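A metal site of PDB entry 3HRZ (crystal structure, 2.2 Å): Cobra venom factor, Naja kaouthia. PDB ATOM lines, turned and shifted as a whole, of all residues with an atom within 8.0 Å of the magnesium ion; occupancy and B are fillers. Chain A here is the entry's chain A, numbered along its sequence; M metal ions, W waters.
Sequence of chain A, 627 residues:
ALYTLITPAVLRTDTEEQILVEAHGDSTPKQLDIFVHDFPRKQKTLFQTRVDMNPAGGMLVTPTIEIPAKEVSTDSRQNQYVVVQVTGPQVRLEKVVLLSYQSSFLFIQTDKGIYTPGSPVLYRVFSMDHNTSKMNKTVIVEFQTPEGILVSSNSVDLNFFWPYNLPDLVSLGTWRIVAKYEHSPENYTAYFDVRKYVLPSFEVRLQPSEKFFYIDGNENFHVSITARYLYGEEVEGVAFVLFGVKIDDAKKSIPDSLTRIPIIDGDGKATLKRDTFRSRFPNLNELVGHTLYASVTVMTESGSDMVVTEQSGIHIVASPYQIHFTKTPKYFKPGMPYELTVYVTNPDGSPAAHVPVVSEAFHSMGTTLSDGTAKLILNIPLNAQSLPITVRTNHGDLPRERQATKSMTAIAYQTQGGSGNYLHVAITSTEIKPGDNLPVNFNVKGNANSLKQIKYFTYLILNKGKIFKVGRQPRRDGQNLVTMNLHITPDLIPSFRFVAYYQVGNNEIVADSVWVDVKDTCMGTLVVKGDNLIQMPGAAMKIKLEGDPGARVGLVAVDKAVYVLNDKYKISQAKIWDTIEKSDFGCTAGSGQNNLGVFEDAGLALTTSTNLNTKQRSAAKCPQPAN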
ATOM      1  N   ILE A 432      20.441 -18.555  -3.574  1.00  0.00           N
ATOM      2  CA  ILE A 432      21.774 -19.085  -3.817  1.00  0.00           C
ATOM      3  C   ILE A 432      22.898 -18.160  -3.348  1.00  0.00           C
ATOM      4  O   ILE A 432      22.847 -16.948  -3.577  1.00  0.00           O
ATOM      5  CB  ILE A 432      21.938 -19.415  -5.305  1.00  0.00           C
ATOM      6  CG1 ILE A 432      20.935 -20.512  -5.699  1.00  0.00           C
ATOM      7  CG2 ILE A 432      23.382 -19.824  -5.613  1.00  0.00           C
ATOM      8  CD1 ILE A 432      20.603 -20.528  -7.128  1.00  0.00           C
ATOM      9  N   LEU A 492      30.532 -15.427  -9.297  1.00  0.00           N
ATOM     10  CA  LEU A 492      29.206 -15.436  -9.913  1.00  0.00           C
ATOM     11  C   LEU A 492      28.251 -14.402  -9.323  1.00  0.00           C
ATOM     12  O   LEU A 492      27.136 -14.238  -9.806  1.00  0.00           O
ATOM     13  CB  LEU A 492      28.582 -16.834  -9.883  1.00  0.00           C
ATOM     14  CG  LEU A 492      29.500 -17.921 -10.447  1.00  0.00           C
ATOM     15  CD1 LEU A 492      28.881 -19.289 -10.260  1.00  0.00           C
ATOM     16  CD2 LEU A 492      29.829 -17.655 -11.920  1.00  0.00           C
ATOM     17  N   ILE A 493      28.705 -13.688  -8.297  1.00  0.00           N
ATOM     18  CA  ILE A 493      27.995 -12.498  -7.809  1.00  0.00           C
ATOM     19  C   ILE A 493      27.975 -11.499  -8.958  1.00  0.00           C
ATOM     20  O   ILE A 493      28.939 -11.407  -9.694  1.00  0.00           O
ATOM     21  CB  ILE A 493      28.752 -11.904  -6.595  1.00  0.00           C
ATOM     22  CG1 ILE A 493      28.767 -12.909  -5.435  1.00  0.00           C
ATOM     23  CG2 ILE A 493      28.172 -10.561  -6.174  1.00  0.00           C
ATOM     24  CD1 ILE A 493      29.840 -12.631  -4.377  1.00  0.00           C
ATOM     25  N   PRO A 494      26.881 -10.742  -9.144  1.00  0.00           N
ATOM     26  CA  PRO A 494      25.620 -10.655  -8.408  1.00  0.00           C
ATOM     27  C   PRO A 494      24.594 -11.638  -8.966  1.00  0.00           C
ATOM     28  O   PRO A 494      23.534 -11.769  -8.369  1.00  0.00           O
ATOM     29  CB  PRO A 494      25.128  -9.253  -8.748  1.00  0.00           C
ATOM     30  CG  PRO A 494      25.757  -8.909 -10.039  1.00  0.00           C
ATOM     31  CD  PRO A 494      26.875  -9.849 -10.312  1.00  0.00           C
ATOM     32  N   SER A 495      24.910 -12.255 -10.105  1.00  0.00           N
ATOM     33  CA  SER A 495      24.035 -13.219 -10.784  1.00  0.00           C
ATOM     34  C   SER A 495      24.791 -13.845 -11.960  1.00  0.00           C
ATOM     35  O   SER A 495      25.873 -13.388 -12.318  1.00  0.00           O
ATOM     36  CB  SER A 495      22.781 -12.526 -11.322  1.00  0.00           C
ATOM     37  OG  SER A 495      23.078 -11.707 -12.454  1.00  0.00           O
ATOM     38  N   PHE A 496      24.233 -14.909 -12.536  1.00  0.00           N
ATOM     39  CA  PHE A 496      24.784 -15.493 -13.756  1.00  0.00           C
ATOM     40  C   PHE A 496      23.741 -16.127 -14.646  1.00  0.00           C
ATOM     41  O   PHE A 496      22.607 -16.378 -14.211  1.00  0.00           O
ATOM     42  CB  PHE A 496      25.876 -16.519 -13.449  1.00  0.00           C
ATOM     43  CG  PHE A 496      25.376 -17.765 -12.749  1.00  0.00           C
ATOM     44  CD1 PHE A 496      25.069 -18.903 -13.467  1.00  0.00           C
ATOM     45  CD2 PHE A 496      25.294 -17.804 -11.362  1.00  0.00           C
ATOM     46  CE1 PHE A 496      24.635 -20.073 -12.822  1.00  0.00           C
ATOM     47  CE2 PHE A 496      24.878 -18.932 -10.714  1.00  0.00           C
ATOM     48  CZ  PHE A 496      24.537 -20.095 -11.441  1.00  0.00           C
ATOM     49  N   TRP A 515      18.376 -17.655 -15.869  1.00  0.00           N
ATOM     50  CA  TRP A 515      19.045 -16.580 -15.127  1.00  0.00           C
ATOM     51  C   TRP A 515      18.976 -16.944 -13.648  1.00  0.00           C
ATOM     52  O   TRP A 515      17.904 -17.253 -13.140  1.00  0.00           O
ATOM     53  CB  TRP A 515      18.375 -15.229 -15.387  1.00  0.00           C
ATOM     54  CG  TRP A 515      18.945 -14.063 -14.576  1.00  0.00           C
ATOM     55  CD1 TRP A 515      20.054 -13.287 -14.898  1.00  0.00           C
ATOM     56  CD2 TRP A 515      18.419 -13.526 -13.359  1.00  0.00           C
ATOM     57  NE1 TRP A 515      20.241 -12.341 -13.935  1.00  0.00           N
ATOM     58  CE2 TRP A 515      19.260 -12.454 -12.983  1.00  0.00           C
ATOM     59  CE3 TRP A 515      17.333 -13.863 -12.538  1.00  0.00           C
ATOM     60  CZ2 TRP A 515      19.043 -11.697 -11.813  1.00  0.00           C
ATOM     61  CZ3 TRP A 515      17.115 -13.115 -11.373  1.00  0.00           C
ATOM     62  CH2 TRP A 515      17.964 -12.040 -11.025  1.00  0.00           C
ATOM     63  N   VAL A 516      20.122 -16.942 -12.991  1.00  0.00           N
ATOM     64  CA  VAL A 516      20.229 -17.345 -11.592  1.00  0.00           C
ATOM     65  C   VAL A 516      20.792 -16.215 -10.734  1.00  0.00           C
ATOM     66  O   VAL A 516      21.926 -15.778 -10.939  1.00  0.00           O
ATOM     67  CB  VAL A 516      21.141 -18.578 -11.429  1.00  0.00           C
ATOM     68  CG1 VAL A 516      21.109 -19.061  -9.991  1.00  0.00           C
ATOM     69  CG2 VAL A 516      20.725 -19.695 -12.372  1.00  0.00           C
ATOM     70  N   ASP A 517      19.997 -15.734  -9.792  1.00  0.00           N
ATOM     71  CA  ASP A 517      20.449 -14.673  -8.902  1.00  0.00           C
ATOM     72  C   ASP A 517      21.395 -15.226  -7.855  1.00  0.00           C
ATOM     73  O   ASP A 517      21.240 -16.353  -7.386  1.00  0.00           O
ATOM     74  CB  ASP A 517      19.247 -14.009  -8.236  1.00  0.00           C
ATOM     75  CG  ASP A 517      19.583 -12.654  -7.569  1.00  0.00           C
ATOM     76  OD1 ASP A 517      20.745 -12.150  -7.608  1.00  0.00           O
ATOM     77  OD2 ASP A 517      18.637 -12.093  -6.974  1.00  0.00           O
ATOM     78  N   VAL A 518      22.395 -14.433  -7.490  1.00  0.00           N
ATOM     79  CA  VAL A 518      23.296 -14.816  -6.430  1.00  0.00           C
ATOM     80  C   VAL A 518      23.227 -13.749  -5.346  1.00  0.00           C
ATOM     81  O   VAL A 518      23.033 -12.547  -5.645  1.00  0.00           O
ATOM     82  CB  VAL A 518      24.722 -15.012  -6.960  1.00  0.00           C
ATOM     83  CG1 VAL A 518      25.691 -15.304  -5.831  1.00  0.00           C
ATOM     84  CG2 VAL A 518      24.757 -16.148  -7.991  1.00  0.00           C
ATOM     85  N   LYS A 519      23.368 -14.171  -4.093  1.00  0.00           N
ATOM     86  CA  LYS A 519      23.325 -13.234  -2.985  1.00  0.00           C
ATOM     87  C   LYS A 519      24.386 -12.156  -3.175  1.00  0.00           C
ATOM     88  O   LYS A 519      25.587 -12.439  -3.288  1.00  0.00           O
ATOM     89  CB  LYS A 519      23.544 -13.948  -1.655  1.00  0.00           C
ATOM     90  CG  LYS A 519      23.149 -13.117  -0.447  1.00  0.00           C
ATOM     91  CD  LYS A 519      24.076 -13.387   0.717  1.00  0.00           C
ATOM     92  CE  LYS A 519      23.779 -12.494   1.910  1.00  0.00           C
ATOM     93  NZ  LYS A 519      22.707 -13.053   2.782  1.00  0.00           N
ATOM     94  N   ASP A 520      23.944 -10.911  -3.211  1.00  0.00           N
ATOM     95  CA  ASP A 520      24.859  -9.802  -3.419  1.00  0.00           C
ATOM     96  C   ASP A 520      25.641  -9.534  -2.133  1.00  0.00           C
ATOM     97  O   ASP A 520      25.068  -9.177  -1.103  1.00  0.00           O
ATOM     98  CB  ASP A 520      24.087  -8.542  -3.822  1.00  0.00           C
ATOM     99  CG  ASP A 520      23.498  -8.639  -5.225  1.00  0.00           C
ATOM    100  OD1 ASP A 520      23.665  -9.670  -5.928  1.00  0.00           O
ATOM    101  OD2 ASP A 520      22.846  -7.641  -5.619  1.00  0.00           O
ATOM    102  N   THR A 521      26.949  -9.768  -2.196  1.00  0.00           N
ATOM    103  CA  THR A 521      27.871  -9.320  -1.160  1.00  0.00           C
ATOM    104  C   THR A 521      29.100  -8.807  -1.899  1.00  0.00           C
ATOM    105  O   THR A 521      29.129  -8.841  -3.134  1.00  0.00           O
ATOM    106  CB  THR A 521      28.289 -10.472  -0.216  1.00  0.00           C
ATOM    107  OG1 THR A 521      29.096 -11.427  -0.936  1.00  0.00           O
ATOM    108  CG2 THR A 521      27.060 -11.194   0.358  1.00  0.00           C
ATOM    109  N   TRP A 577      26.598  -3.343  -7.488  1.00  0.00           N
ATOM    110  CA  TRP A 577      25.925  -4.469  -8.130  1.00  0.00           C
ATOM    111  C   TRP A 577      24.783  -4.003  -9.047  1.00  0.00           C
ATOM    112  O   TRP A 577      24.624  -4.501 -10.152  1.00  0.00           O
ATOM    113  CB  TRP A 577      25.454  -5.502  -7.110  1.00  0.00           C
ATOM    114  CG  TRP A 577      26.592  -6.101  -6.350  1.00  0.00           C
ATOM    115  CD1 TRP A 577      26.715  -6.221  -4.994  1.00  0.00           C
ATOM    116  CD2 TRP A 577      27.809  -6.640  -6.910  1.00  0.00           C
ATOM    117  NE1 TRP A 577      27.929  -6.812  -4.681  1.00  0.00           N
ATOM    118  CE2 TRP A 577      28.609  -7.071  -5.838  1.00  0.00           C
ATOM    119  CE3 TRP A 577      28.284  -6.802  -8.218  1.00  0.00           C
ATOM    120  CZ2 TRP A 577      29.864  -7.656  -6.022  1.00  0.00           C
ATOM    121  CZ3 TRP A 577      29.526  -7.383  -8.405  1.00  0.00           C
ATOM    122  CH2 TRP A 577      30.306  -7.804  -7.304  1.00  0.00           C
ATOM    123  N   GLU A 581      24.352  -4.906 -12.996  1.00  0.00           N
ATOM    124  CA  GLU A 581      23.168  -5.601 -13.539  1.00  0.00           C
ATOM    125  C   GLU A 581      22.517  -4.791 -14.654  1.00  0.00           C
ATOM    126  O   GLU A 581      22.089  -5.339 -15.657  1.00  0.00           O
ATOM    127  CB  GLU A 581      22.117  -5.882 -12.445  1.00  0.00           C
ATOM    128  CG  GLU A 581      22.532  -6.874 -11.351  1.00  0.00           C
ATOM    129  CD  GLU A 581      22.602  -8.315 -11.838  1.00  0.00           C
ATOM    130  OE1 GLU A 581      22.898  -8.528 -13.044  1.00  0.00           O
ATOM    131  OE2 GLU A 581      22.375  -9.246 -11.031  1.00  0.00           O
HETATM  132 MG    MG M   1      22.317 -11.000  -6.845  1.00  0.00          MG
HETATM  133  O   HOH W   1      20.981 -10.202  -5.470  1.00  0.00           O
HETATM  134  O   HOH W   2      21.764  -9.572  -8.269  1.00  0.00           O
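The magnesium ion is bound by water W1 (2.1 Å). O of Val 518 binds the magnesium ion. Water W2 is bound to the magnesium ion (2.1 Å). The side-chain carboxylate (OD1) of Asp 517 is bound to the magnesium ion. The magnesium ion is bound by O of Pro 494 (2.1 Å). The side-chain carboxylate (OD1) of Asp 520 is bound to the magnesium ion (2.1 Å).
Water W2 bridges the side-chain carboxylate of Glu 581 and the side-chain carboxylate of Asp 520. Water W1 lies within hydrogen-bond range of OD2 of Asp 520 (3.2 Å) and OD2 of Asp 517 (3.4 Å).
Within 4 Å of the magnesium ion: Pro 494, Asp 517, Val 518 and Asp 520. Along chain A the residues within 4 Å of the magnesium ion span positions 494 to 520. The nearest printed residue that does not touch the magnesium ion is Lys 519 (4.3 Å).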
